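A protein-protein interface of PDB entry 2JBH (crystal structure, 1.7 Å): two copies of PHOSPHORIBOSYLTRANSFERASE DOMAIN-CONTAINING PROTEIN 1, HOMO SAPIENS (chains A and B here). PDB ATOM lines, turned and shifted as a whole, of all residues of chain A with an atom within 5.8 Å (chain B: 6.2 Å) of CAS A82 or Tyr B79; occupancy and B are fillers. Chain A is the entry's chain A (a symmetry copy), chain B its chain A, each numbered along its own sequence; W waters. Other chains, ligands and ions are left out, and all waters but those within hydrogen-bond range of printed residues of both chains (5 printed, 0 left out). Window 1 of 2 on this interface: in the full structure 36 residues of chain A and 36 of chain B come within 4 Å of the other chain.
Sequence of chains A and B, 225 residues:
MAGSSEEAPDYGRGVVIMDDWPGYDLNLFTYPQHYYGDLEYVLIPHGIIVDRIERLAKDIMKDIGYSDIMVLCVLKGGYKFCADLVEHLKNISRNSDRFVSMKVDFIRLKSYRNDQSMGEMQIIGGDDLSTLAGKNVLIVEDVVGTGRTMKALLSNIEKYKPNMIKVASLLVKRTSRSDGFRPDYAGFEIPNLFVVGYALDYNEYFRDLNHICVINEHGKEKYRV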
ATOM      1  N   VAL A  71     -12.811  29.827  -1.960  1.00  0.00           N
ATOM      2  CA  VAL A  71     -13.239  28.841  -0.964  1.00  0.00           C
ATOM      3  C   VAL A  71     -12.942  27.471  -1.530  1.00  0.00           C
ATOM      4  O   VAL A  71     -13.353  27.161  -2.652  1.00  0.00           O
ATOM      5  CB  VAL A  71     -14.753  28.963  -0.653  1.00  0.00           C
ATOM      6  CG1 VAL A  71     -15.190  27.869   0.320  1.00  0.00           C
ATOM      7  CG2 VAL A  71     -15.088  30.353  -0.089  1.00  0.00           C
ATOM      8  N   LEU A  72     -12.240  26.645  -0.756  1.00  0.00           N
ATOM      9  CA  LEU A  72     -11.899  25.305  -1.203  1.00  0.00           C
ATOM     10  C   LEU A  72     -12.513  24.296  -0.223  1.00  0.00           C
ATOM     11  O   LEU A  72     -12.033  24.130   0.899  1.00  0.00           O
ATOM     12  CB  LEU A  72     -10.390  25.179  -1.257  1.00  0.00           C
ATOM     13  CG  LEU A  72      -9.712  23.934  -1.801  1.00  0.00           C
ATOM     14  CD1 LEU A  72     -10.108  23.633  -3.237  1.00  0.00           C
ATOM     15  CD2 LEU A  72      -8.197  24.196  -1.726  1.00  0.00           C
ATOM     16  N   CYS A  73     -13.607  23.677  -0.660  1.00  0.00           N
ATOM     17  CA  CYS A  73     -14.362  22.733   0.158  1.00  0.00           C
ATOM     18  C   CYS A  73     -13.717  21.352   0.123  1.00  0.00           C
ATOM     19  O   CYS A  73     -13.535  20.800  -0.957  1.00  0.00           O
ATOM     20  CB  CYS A  73     -15.766  22.604  -0.406  1.00  0.00           C
ATOM     21  SG  CYS A  73     -16.793  21.486   0.518  1.00  0.00           S
ATOM     22  N   GLY A  78     -16.865  18.046   4.429  1.00  0.00           N
ATOM     23  CA  GLY A  78     -16.889  19.512   4.566  1.00  0.00           C
ATOM     24  C   GLY A  78     -18.096  20.200   3.948  1.00  0.00           C
ATOM     25  O   GLY A  78     -18.258  21.427   4.145  1.00  0.00           O
ATOM     26  N   TYR A  79     -18.938  19.474   3.208  1.00  0.00           N
ATOM     27  CA  TYR A  79     -19.920  20.154   2.314  1.00  0.00           C
ATOM     28  C   TYR A  79     -20.949  20.992   3.070  1.00  0.00           C
ATOM     29  O   TYR A  79     -21.261  22.113   2.657  1.00  0.00           O
ATOM     30  CB  TYR A  79     -20.573  19.206   1.277  1.00  0.00           C
ATOM     31  CG  TYR A  79     -22.013  18.843   1.563  1.00  0.00           C
ATOM     32  CD1 TYR A  79     -22.332  17.608   2.120  1.00  0.00           C
ATOM     33  CD2 TYR A  79     -23.061  19.751   1.311  1.00  0.00           C
ATOM     34  CE1 TYR A  79     -23.669  17.263   2.414  1.00  0.00           C
ATOM     35  CE2 TYR A  79     -24.411  19.420   1.598  1.00  0.00           C
ATOM     36  CZ  TYR A  79     -24.694  18.180   2.159  1.00  0.00           C
ATOM     37  OH  TYR A  79     -25.987  17.861   2.466  1.00  0.00           O
ATOM     38  N   LYS A  80     -21.442  20.491   4.199  1.00  0.00           N
ATOM     39  CA  LYS A  80     -22.494  21.218   4.924  1.00  0.00           C
ATOM     40  C   LYS A  80     -21.938  22.450   5.622  1.00  0.00           C
ATOM     41  O   LYS A  80     -22.520  23.550   5.519  1.00  0.00           O
ATOM     42  CB  LYS A  80     -23.173  20.295   5.936  1.00  0.00           C
ATOM     43  CG  LYS A  80     -24.509  19.784   5.516  1.00  0.00           C
ATOM     44  CD  LYS A  80     -25.650  20.633   6.125  1.00  0.00           C
ATOM     45  CE  LYS A  80     -25.724  22.033   5.566  1.00  0.00           C
ATOM     46  NZ  LYS A  80     -27.085  22.669   5.721  1.00  0.00           N
ATOM     47  N   PHE A  81     -20.828  22.265   6.336  1.00  0.00           N
ATOM     48  CA  PHE A  81     -20.136  23.396   6.985  1.00  0.00           C
ATOM     49  C   PHE A  81     -19.781  24.479   5.962  1.00  0.00           C
ATOM     50  O   PHE A  81     -20.126  25.672   6.142  1.00  0.00           O
ATOM     51  CB  PHE A  81     -18.868  22.861   7.633  1.00  0.00           C
ATOM     52  CG  PHE A  81     -17.980  23.915   8.273  1.00  0.00           C
ATOM     53  CD1 PHE A  81     -18.500  25.019   8.955  1.00  0.00           C
ATOM     54  CD2 PHE A  81     -16.596  23.745   8.230  1.00  0.00           C
ATOM     55  CE1 PHE A  81     -17.640  25.957   9.575  1.00  0.00           C
ATOM     56  CE2 PHE A  81     -15.737  24.675   8.845  1.00  0.00           C
ATOM     57  CZ  PHE A  81     -16.261  25.789   9.498  1.00  0.00           C
ATOM     58  N   CAS A  82     -19.206  24.023   4.694  1.00  0.00           N
ATOM     59  CA  CAS A  82     -18.827  24.969   3.631  1.00  0.00           C
ATOM     60  CB  CAS A  82     -18.260  24.151   2.493  1.00  0.00           C
ATOM     61  C   CAS A  82     -20.068  25.692   3.174  1.00  0.00           C
ATOM     62  O   CAS A  82     -20.207  26.944   3.191  1.00  0.00           O
ATOM     63  SG  CAS A  82     -17.839  25.239   1.141  1.00  0.00           S
ATOM     64 AS   CAS A  82     -19.759  25.393  -0.052  1.00  0.00          AS
ATOM     65  CE1 CAS A  82     -20.206  23.480  -0.306  1.00  0.00           C
ATOM     66  CE2 CAS A  82     -19.061  25.928  -1.815  1.00  0.00           C
ATOM     67  N   ALA A  83     -21.323  24.833   2.856  1.00  0.00           N
ATOM     68  CA  ALA A  83     -22.561  25.485   2.331  1.00  0.00           C
ATOM     69  C   ALA A  83     -23.038  26.549   3.312  1.00  0.00           C
ATOM     70  O   ALA A  83     -23.337  27.692   2.909  1.00  0.00           O
ATOM     71  CB  ALA A  83     -23.641  24.430   2.096  1.00  0.00           C
ATOM     72  N   ASP A  84     -23.076  26.207   4.600  1.00  0.00           N
ATOM     73  CA  ASP A  84     -23.603  27.136   5.594  1.00  0.00           C
ATOM     74  C   ASP A  84     -22.685  28.338   5.848  1.00  0.00           C
ATOM     75  O   ASP A  84     -23.172  29.463   6.009  1.00  0.00           O
ATOM     76  CB  ASP A  84     -23.906  26.410   6.898  1.00  0.00           C
ATOM     77  CG  ASP A  84     -25.154  25.522   6.814  1.00  0.00           C
ATOM     78  OD1 ASP A  84     -25.863  25.532   5.780  1.00  0.00           O
ATOM     79  OD2 ASP A  84     -25.454  24.848   7.825  1.00  0.00           O
ATOM     80  N   LEU A  85     -21.379  28.104   5.846  1.00  0.00           N
ATOM     81  CA  LEU A  85     -20.405  29.162   6.076  1.00  0.00           C
ATOM     82  C   LEU A  85     -20.503  30.154   4.908  1.00  0.00           C
ATOM     83  O   LEU A  85     -20.576  31.374   5.122  1.00  0.00           O
ATOM     84  CB  LEU A  85     -18.991  28.588   6.195  1.00  0.00           C
ATOM     85  CG  LEU A  85     -17.879  29.603   6.407  1.00  0.00           C
ATOM     86  CD1 LEU A  85     -18.100  30.366   7.716  1.00  0.00           C
ATOM     87  CD2 LEU A  85     -16.523  28.878   6.429  1.00  0.00           C
ATOM     88  N   VAL A  86     -20.542  29.622   3.690  1.00  0.00           N
ATOM     89  CA  VAL A  86     -20.714  30.453   2.464  1.00  0.00           C
ATOM     90  C   VAL A  86     -22.020  31.261   2.533  1.00  0.00           C
ATOM     91  O   VAL A  86     -22.037  32.460   2.225  1.00  0.00           O
ATOM     92  CB  VAL A  86     -20.569  29.596   1.183  1.00  0.00           C
ATOM     93  CG1 VAL A  86     -20.972  30.381  -0.085  1.00  0.00           C
ATOM     94  CG2 VAL A  86     -19.101  29.122   1.041  1.00  0.00           C
ATOM     95  N   GLU A  87     -23.116  30.628   2.955  1.00  0.00           N
ATOM     96  CA  GLU A  87     -24.378  31.373   3.099  1.00  0.00           C
ATOM     97  C   GLU A  87     -24.249  32.534   4.068  1.00  0.00           C
ATOM     98  O   GLU A  87     -24.808  33.628   3.832  1.00  0.00           O
ATOM     99  CB  GLU A  87     -25.509  30.450   3.519  1.00  0.00           C
ATOM    100  CG  GLU A  87     -25.967  29.512   2.414  1.00  0.00           C
ATOM    101  CD  GLU A  87     -26.308  30.247   1.122  1.00  0.00           C
ATOM    102  OE1 GLU A  87     -27.189  31.127   1.154  1.00  0.00           O
ATOM    103  OE2 GLU A  87     -25.663  29.957   0.105  1.00  0.00           O
ATOM    104  N   LYS A  90     -22.240  35.206   2.429  1.00  0.00           N
ATOM    105  CA  LYS A  90     -23.095  35.829   1.416  1.00  0.00           C
ATOM    106  C   LYS A  90     -24.059  36.821   2.096  1.00  0.00           C
ATOM    107  O   LYS A  90     -24.248  37.954   1.638  1.00  0.00           O
ATOM    108  CB  LYS A  90     -23.896  34.761   0.653  1.00  0.00           C
ATOM    109  CG  LYS A  90     -23.076  34.064  -0.419  1.00  0.00           C
ATOM    110  CD  LYS A  90     -23.685  32.743  -0.887  1.00  0.00           C
ATOM    111  CE  LYS A  90     -25.109  32.880  -1.331  1.00  0.00           C
ATOM    112  NZ  LYS A  90     -25.722  31.604  -1.835  1.00  0.00           N
ATOM    113  N   VAL A 104     -15.782  29.422  -5.582  1.00  0.00           N
ATOM    114  CA  VAL A 104     -15.808  28.169  -4.812  1.00  0.00           C
ATOM    115  C   VAL A 104     -15.222  27.040  -5.622  1.00  0.00           C
ATOM    116  O   VAL A 104     -15.373  26.998  -6.845  1.00  0.00           O
ATOM    117  CB  VAL A 104     -17.227  27.799  -4.353  1.00  0.00           C
ATOM    118  CG1 VAL A 104     -17.807  28.925  -3.505  1.00  0.00           C
ATOM    119  CG2 VAL A 104     -18.131  27.464  -5.533  1.00  0.00           C
ATOM    120  N   ASP A 105     -14.557  26.120  -4.934  1.00  0.00           N
ATOM    121  CA  ASP A 105     -14.063  24.904  -5.584  1.00  0.00           C
ATOM    122  C   ASP A 105     -14.155  23.772  -4.592  1.00  0.00           C
ATOM    123  O   ASP A 105     -14.436  23.996  -3.413  1.00  0.00           O
ATOM    124  CB  ASP A 105     -12.630  25.058  -6.062  1.00  0.00           C
ATOM    125  CG  ASP A 105     -12.209  23.980  -7.079  1.00  0.00           C
ATOM    126  OD1 ASP A 105     -13.057  23.212  -7.651  1.00  0.00           O
ATOM    127  OD2 ASP A 105     -10.987  23.916  -7.314  1.00  0.00           O
ATOM    128  N   PHE A 106     -13.906  22.565  -5.081  1.00  0.00           N
ATOM    129  CA  PHE A 106     -14.204  21.364  -4.305  1.00  0.00           C
ATOM    130  C   PHE A 106     -13.128  20.357  -4.586  1.00  0.00           C
ATOM    131  O   PHE A 106     -12.806  20.086  -5.756  1.00  0.00           O
ATOM    132  CB  PHE A 106     -15.533  20.745  -4.753  1.00  0.00           C
ATOM    133  CG  PHE A 106     -16.712  21.685  -4.698  1.00  0.00           C
ATOM    134  CD1 PHE A 106     -16.989  22.547  -5.763  1.00  0.00           C
ATOM    135  CD2 PHE A 106     -17.565  21.679  -3.601  1.00  0.00           C
ATOM    136  CE1 PHE A 106     -18.064  23.397  -5.732  1.00  0.00           C
ATOM    137  CE2 PHE A 106     -18.670  22.509  -3.565  1.00  0.00           C
ATOM    138  CZ  PHE A 106     -18.910  23.395  -4.636  1.00  0.00           C
ATOM    139  N   VAL A 140     -11.994  24.636   3.717  1.00  0.00           N
ATOM    140  CA  VAL A 140     -13.121  24.384   4.627  1.00  0.00           C
ATOM    141  C   VAL A 140     -13.221  22.878   4.840  1.00  0.00           C
ATOM    142  O   VAL A 140     -13.494  22.135   3.891  1.00  0.00           O
ATOM    143  CB  VAL A 140     -14.456  24.918   4.066  1.00  0.00           C
ATOM    144  CG1 VAL A 140     -15.615  24.612   5.034  1.00  0.00           C
ATOM    145  CG2 VAL A 140     -14.374  26.476   3.800  1.00  0.00           C
ATOM    146  N   CYS B  73     -24.582  14.884  -6.975  1.00  0.00           N
ATOM    147  CA  CYS B  73     -24.519  16.313  -7.266  1.00  0.00           C
ATOM    148  C   CYS B  73     -23.582  16.585  -8.437  1.00  0.00           C
ATOM    149  O   CYS B  73     -22.420  16.197  -8.381  1.00  0.00           O
ATOM    150  CB  CYS B  73     -23.968  17.039  -6.051  1.00  0.00           C
ATOM    151  SG  CYS B  73     -23.856  18.799  -6.277  1.00  0.00           S
ATOM    152  N   VAL B  74     -24.068  17.298  -9.465  1.00  0.00           N
ATOM    153  CA  VAL B  74     -23.218  17.674 -10.594  1.00  0.00           C
ATOM    154  C   VAL B  74     -22.571  19.049 -10.313  1.00  0.00           C
ATOM    155  O   VAL B  74     -23.206  20.095 -10.490  1.00  0.00           O
ATOM    156  CB  VAL B  74     -23.993  17.724 -11.933  1.00  0.00           C
ATOM    157  CG1 VAL B  74     -23.008  17.906 -13.088  1.00  0.00           C
ATOM    158  CG2 VAL B  74     -24.816  16.413 -12.131  1.00  0.00           C
ATOM    159  N   LEU B  75     -21.347  19.005  -9.801  1.00  0.00           N
ATOM    160  CA  LEU B  75     -20.562  20.199  -9.467  1.00  0.00           C
ATOM    161  C   LEU B  75     -20.115  20.937 -10.757  1.00  0.00           C
ATOM    162  O   LEU B  75     -20.030  20.319 -11.812  1.00  0.00           O
ATOM    163  CB  LEU B  75     -19.318  19.795  -8.674  1.00  0.00           C
ATOM    164  CG  LEU B  75     -19.527  19.225  -7.281  1.00  0.00           C
ATOM    165  CD1 LEU B  75     -18.185  18.714  -6.746  1.00  0.00           C
ATOM    166  CD2 LEU B  75     -20.139  20.252  -6.384  1.00  0.00           C
ATOM    167  N   LYS B  76     -19.823  22.243 -10.675  1.00  0.00           N
ATOM    168  CA  LYS B  76     -20.013  23.046  -9.458  1.00  0.00           C
ATOM    169  C   LYS B  76     -21.409  23.659  -9.385  1.00  0.00           C
ATOM    170  O   LYS B  76     -21.916  23.939  -8.294  1.00  0.00           O
ATOM    171  CB  LYS B  76     -19.017  24.215  -9.429  1.00  0.00           C
ATOM    172  CG  LYS B  76     -17.566  23.841  -9.624  1.00  0.00           C
ATOM    173  CD  LYS B  76     -16.751  25.149  -9.484  1.00  0.00           C
ATOM    174  CE  LYS B  76     -15.301  24.959  -9.706  1.00  0.00           C
ATOM    175  NZ  LYS B  76     -14.573  26.260  -9.575  1.00  0.00           N
ATOM    176  N   GLY B  77     -22.015  23.890 -10.547  1.00  0.00           N
ATOM    177  CA  GLY B  77     -23.280  24.635 -10.643  1.00  0.00           C
ATOM    178  C   GLY B  77     -24.443  23.995  -9.897  1.00  0.00           C
ATOM    179  O   GLY B  77     -25.355  24.690  -9.499  1.00  0.00           O
ATOM    180  N   GLY B  78     -24.405  22.674  -9.715  1.00  0.00           N
ATOM    181  CA  GLY B  78     -25.497  21.990  -9.001  1.00  0.00           C
ATOM    182  C   GLY B  78     -25.465  22.125  -7.487  1.00  0.00           C
ATOM    183  O   GLY B  78     -26.434  21.691  -6.822  1.00  0.00           O
ATOM    184  N   TYR B  79     -24.401  22.696  -6.917  1.00  0.00           N
ATOM    185  CA  TYR B  79     -24.169  22.541  -5.451  1.00  0.00           C
ATOM    186  C   TYR B  79     -25.255  23.185  -4.594  1.00  0.00           C
ATOM    187  O   TYR B  79     -25.699  22.593  -3.605  1.00  0.00           O
ATOM    188  CB  TYR B  79     -22.741  22.946  -5.004  1.00  0.00           C
ATOM    189  CG  TYR B  79     -22.656  24.259  -4.257  1.00  0.00           C
ATOM    190  CD1 TYR B  79     -22.220  25.412  -4.904  1.00  0.00           C
ATOM    191  CD2 TYR B  79     -23.049  24.359  -2.906  1.00  0.00           C
ATOM    192  CE1 TYR B  79     -22.156  26.648  -4.227  1.00  0.00           C
ATOM    193  CE2 TYR B  79     -22.990  25.594  -2.210  1.00  0.00           C
ATOM    194  CZ  TYR B  79     -22.554  26.727  -2.887  1.00  0.00           C
ATOM    195  OH  TYR B  79     -22.519  27.929  -2.235  1.00  0.00           O
ATOM    196  N   LYS B  80     -25.730  24.364  -4.984  1.00  0.00           N
ATOM    197  CA  LYS B  80     -26.719  25.066  -4.154  1.00  0.00           C
ATOM    198  C   LYS B  80     -28.086  24.402  -4.234  1.00  0.00           C
ATOM    199  O   LYS B  80     -28.732  24.163  -3.195  1.00  0.00           O
ATOM    200  CB  LYS B  80     -26.816  26.533  -4.575  1.00  0.00           C
ATOM    201  CG  LYS B  80     -26.115  27.489  -3.670  1.00  0.00           C
ATOM    202  CD  LYS B  80     -27.098  28.127  -2.660  1.00  0.00           C
ATOM    203  CE  LYS B  80     -27.630  27.152  -1.639  1.00  0.00           C
ATOM    204  NZ  LYS B  80     -28.127  27.817  -0.377  1.00  0.00           N
ATOM    205  N   PHE B  81     -28.525  24.117  -5.460  1.00  0.00           N
ATOM    206  CA  PHE B  81     -29.791  23.388  -5.672  1.00  0.00           C
ATOM    207  C   PHE B  81     -29.782  22.051  -4.925  1.00  0.00           C
ATOM    208  O   PHE B  81     -30.710  21.749  -4.135  1.00  0.00           O
ATOM    209  CB  PHE B  81     -29.950  23.146  -7.165  1.00  0.00           C
ATOM    210  CG  PHE B  81     -31.164  22.321  -7.555  1.00  0.00           C
ATOM    211  CD1 PHE B  81     -32.395  22.443  -6.903  1.00  0.00           C
ATOM    212  CD2 PHE B  81     -31.066  21.453  -8.642  1.00  0.00           C
ATOM    213  CE1 PHE B  81     -33.515  21.687  -7.324  1.00  0.00           C
ATOM    214  CE2 PHE B  81     -32.176  20.699  -9.066  1.00  0.00           C
ATOM    215  CZ  PHE B  81     -33.393  20.804  -8.392  1.00  0.00           C
ATOM    216  N   CAS B  82     -28.561  21.249  -5.027  1.00  0.00           N
ATOM    217  CA  CAS B  82     -28.431  19.945  -4.352  1.00  0.00           C
ATOM    218  CB  CAS B  82     -27.061  19.406  -4.691  1.00  0.00           C
ATOM    219  C   CAS B  82     -28.541  20.170  -2.864  1.00  0.00           C
ATOM    220  O   CAS B  82     -29.395  19.613  -2.125  1.00  0.00           O
ATOM    221  SG  CAS B  82     -26.817  17.852  -3.846  1.00  0.00           S
ATOM    222 AS   CAS B  82     -25.976  18.455  -1.830  1.00  0.00          AS
ATOM    223  CE1 CAS B  82     -24.480  19.633  -2.376  1.00  0.00           C
ATOM    224  CE2 CAS B  82     -25.064  16.792  -1.294  1.00  0.00           C
ATOM    225  N   ALA B  83     -27.682  21.306  -2.244  1.00  0.00           N
ATOM    226  CA  ALA B  83     -27.694  21.530  -0.766  1.00  0.00           C
ATOM    227  C   ALA B  83     -29.119  21.798  -0.298  1.00  0.00           C
ATOM    228  O   ALA B  83     -29.584  21.191   0.688  1.00  0.00           O
ATOM    229  CB  ALA B  83     -26.770  22.694  -0.413  1.00  0.00           C
ATOM    230  N   ASP B  84     -29.834  22.667  -1.012  1.00  0.00           N
ATOM    231  CA  ASP B  84     -31.176  23.047  -0.581  1.00  0.00           C
ATOM    232  C   ASP B  84     -32.207  21.924  -0.748  1.00  0.00           C
ATOM    233  O   ASP B  84     -33.069  21.745   0.120  1.00  0.00           O
ATOM    234  CB  ASP B  84     -31.634  24.306  -1.305  1.00  0.00           C
ATOM    235  CG  ASP B  84     -30.928  25.574  -0.807  1.00  0.00           C
ATOM    236  OD1 ASP B  84     -30.149  25.515   0.174  1.00  0.00           O
ATOM    237  OD2 ASP B  84     -31.205  26.653  -1.377  1.00  0.00           O
ATOM    238  N   PHE B 106     -20.566  13.393  -5.387  1.00  0.00           N
ATOM    239  CA  PHE B 106     -20.315  14.627  -6.128  1.00  0.00           C
ATOM    240  C   PHE B 106     -19.464  14.283  -7.316  1.00  0.00           C
ATOM    241  O   PHE B 106     -18.430  13.605  -7.179  1.00  0.00           O
ATOM    242  CB  PHE B 106     -19.520  15.619  -5.273  1.00  0.00           C
ATOM    243  CG  PHE B 106     -20.155  15.951  -3.945  1.00  0.00           C
ATOM    244  CD1 PHE B 106     -19.945  15.134  -2.829  1.00  0.00           C
ATOM    245  CD2 PHE B 106     -20.928  17.096  -3.802  1.00  0.00           C
ATOM    246  CE1 PHE B 106     -20.504  15.430  -1.613  1.00  0.00           C
ATOM    247  CE2 PHE B 106     -21.478  17.425  -2.577  1.00  0.00           C
ATOM    248  CZ  PHE B 106     -21.280  16.568  -1.472  1.00  0.00           C
ATOM    249  N   VAL B 140     -28.506  15.545  -9.589  1.00  0.00           N
ATOM    250  CA  VAL B 140     -28.967  16.909  -9.289  1.00  0.00           C
ATOM    251  C   VAL B 140     -28.102  17.879 -10.085  1.00  0.00           C
ATOM    252  O   VAL B 140     -26.892  17.965  -9.851  1.00  0.00           O
ATOM    253  CB  VAL B 140     -28.869  17.242  -7.785  1.00  0.00           C
ATOM    254  CG1 VAL B 140     -29.334  18.686  -7.515  1.00  0.00           C
ATOM    255  CG2 VAL B 140     -29.729  16.229  -6.925  1.00  0.00           C
ATOM    256  N   TYR B 198     -27.099  31.616  -7.756  1.00  0.00           N
ATOM    257  CA  TYR B 198     -27.525  30.374  -7.085  1.00  0.00           C
ATOM    258  C   TYR B 198     -26.584  29.231  -7.520  1.00  0.00           C
ATOM    259  O   TYR B 198     -27.031  28.129  -7.878  1.00  0.00           O
ATOM    260  CB  TYR B 198     -28.994  30.082  -7.419  1.00  0.00           C
ATOM    261  CG  TYR B 198     -29.653  29.075  -6.499  1.00  0.00           C
ATOM    262  CD1 TYR B 198     -30.027  29.427  -5.199  1.00  0.00           C
ATOM    263  CD2 TYR B 198     -29.896  27.788  -6.935  1.00  0.00           C
ATOM    264  CE1 TYR B 198     -30.623  28.478  -4.341  1.00  0.00           C
ATOM    265  CE2 TYR B 198     -30.517  26.850  -6.111  1.00  0.00           C
ATOM    266  CZ  TYR B 198     -30.861  27.191  -4.825  1.00  0.00           C
ATOM    267  OH  TYR B 198     -31.464  26.220  -4.030  1.00  0.00           O
ATOM    268  N   ALA B 199     -25.287  29.533  -7.453  1.00  0.00           N
ATOM    269  CA  ALA B 199     -24.163  28.636  -7.779  1.00  0.00           C
ATOM    270  C   ALA B 199     -23.809  28.579  -9.257  1.00  0.00           C
ATOM    271  O   ALA B 199     -22.736  28.076  -9.593  1.00  0.00           O
ATOM    272  CB  ALA B 199     -24.340  27.206  -7.225  1.00  0.00           C
ATOM    273  N   ARG B 207     -21.304  32.793  -8.585  1.00  0.00           N
ATOM    274  CA  ARG B 207     -21.798  31.629  -7.849  1.00  0.00           C
ATOM    275  C   ARG B 207     -22.356  32.038  -6.478  1.00  0.00           C
ATOM    276  O   ARG B 207     -23.196  31.336  -5.925  1.00  0.00           O
ATOM    277  CB  ARG B 207     -20.726  30.575  -7.663  1.00  0.00           C
ATOM    278  CG  ARG B 207     -20.126  30.080  -8.965  1.00  0.00           C
ATOM    279  CD  ARG B 207     -19.477  28.720  -8.765  1.00  0.00           C
ATOM    280  NE  ARG B 207     -18.673  28.312  -9.917  1.00  0.00           N
ATOM    281  CZ  ARG B 207     -19.114  27.574 -10.942  1.00  0.00           C
ATOM    282  NH1 ARG B 207     -20.390  27.247 -11.033  1.00  0.00           N
ATOM    283  NH2 ARG B 207     -18.278  27.213 -11.918  1.00  0.00           N
HETATM  284  O   HOH W   1     -23.476  30.285  -3.439  1.00  0.00           O
HETATM  285  O   HOH W   2     -27.793  19.879   2.389  1.00  0.00           O
HETATM  286  O   HOH W   3     -23.764  28.047   0.167  1.00  0.00           O
HETATM  287  O   HOH W   4     -13.598  28.969  -8.786  1.00  0.00           O
HETATM  288  O   HOH W   5     -16.421  29.868  -8.506  1.00  0.00           O
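The side-chain amino group (NZ) of Lys B80 lies within salt-bridge range of the side-chain carboxylate (OE2) of Glu A87 (3.3 Å). O of Val A104 sits at hydrogen-bond distance from NZ of Lys B76, at 2.9 Å. The side-chain amino group (NZ) of Lys B76 lies within salt-bridge range of the side-chain carboxylate (OD1) of Asp A105 (3.9 Å).
The backbone NH (N) of Cys A73 lies within hydrogen-bond range of the backbone carbonyl oxygen (O) of Asp A105 (2.9 Å). The guanidinium group of Arg B207 sits at hydrogen-bond distance from the backbone carbonyl oxygen of Ala B199 (2.9 Å). The side-chain amino group (NZ) of Lys B80 is in salt-bridge range of the side-chain carboxylate (OD1) of Asp B84 (3.1 Å). The backbone carbonyl oxygen (O) of Val A71 sits at hydrogen-bond distance from the backbone NH (N) of Asp A105, 2.8 Å away. The side-chain amino group (NZ) of Lys A90 lies within salt-bridge range of the side-chain carboxylate (OE2) of Glu A87 (2.5 Å).
Among the printed residues, merely in contact across the chains: Tyr A79 with CAS B82 (3.7 Å), Tyr A79 with Phe B106 (3.9 Å), CAS A82 with Tyr B79 (3.7 Å), Val A86 with Tyr B79 (3.6 Å), Lys A90 with Lys B80 (3.8 Å), Val A104 with Arg B207 (3.7 Å), Phe A106 with Leu B75 (3.8 Å), Phe A106 with Lys B76 (3.9 Å) and Phe A106 with Tyr B79 (3.9 Å).
Tyr B79 touches just these residues of chain A: CAS A82 (3.7 Å), Val A86 (3.6 Å) and Phe A106 (3.9 Å). Of the printed residues of chain A, Lys B76 touches Val A104 (2.9 Å), Asp A105 (3.5 Å) and Phe A106 (3.9 Å). Of the printed residues of chain A, Leu B75 touches Phe A106. Of the printed residues of chain B, Phe A106 touches Leu B75 (3.8 Å), Lys B76 (3.9 Å) and Tyr B79 (3.9 Å). Of the printed residues of chain B, Lys A90 touches Lys B80 (3.8 Å). Of the printed residues of chain A, Lys B80 touches Glu A87 and Lys A90. The nearest residue of chain B that does not touch CAS A82 is CAS B82 (6.1 Å). The nearest printed residue of chain A that does not touch Lys B80 is Ala A83 (5.8 Å).
Of the 17 printed residues of chain B, 7 touch a printed residue of chain A. Of the 18 printed residues of chain A, 8 touch a printed residue of chain B. Among the printed residues, Asp or Glu carboxylates within 4 Å of a Lys or Arg side-chain nitrogen of the other chain: Glu A87 with Lys B80 (3.3 Å) and Asp A105 with Lys B76 (3.9 Å).
Tyr A79 touches CAS B82, and with the chains exchanged CAS A82 touches Tyr B79. Tyr A79 touches Phe B106, and with the chains exchanged Phe A106 touches Tyr B79.
Water W3 lies within hydrogen-bond range of OE2 of Glu A87, OH of Tyr B79 and O of Ala A83. Water W2 bridges OH of Tyr A79 (2.7 Å) and O of Ala B83 (2.8 Å). Water W1 lies within hydrogen-bond range of the backbone carbonyl oxygen (O) of Arg B207 (2.7 Å), the side-chain hydroxyl (OH) of Tyr B79 (2.8 Å) and the side-chain amino group (NZ) of Lys A90 (3.1 Å). Water W4 lies within hydrogen-bond range of NZ of Lys B76 and O of Val A104. Water W5 bridges the backbone NH of Val A104 and the guanidinium group of Arg B207.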
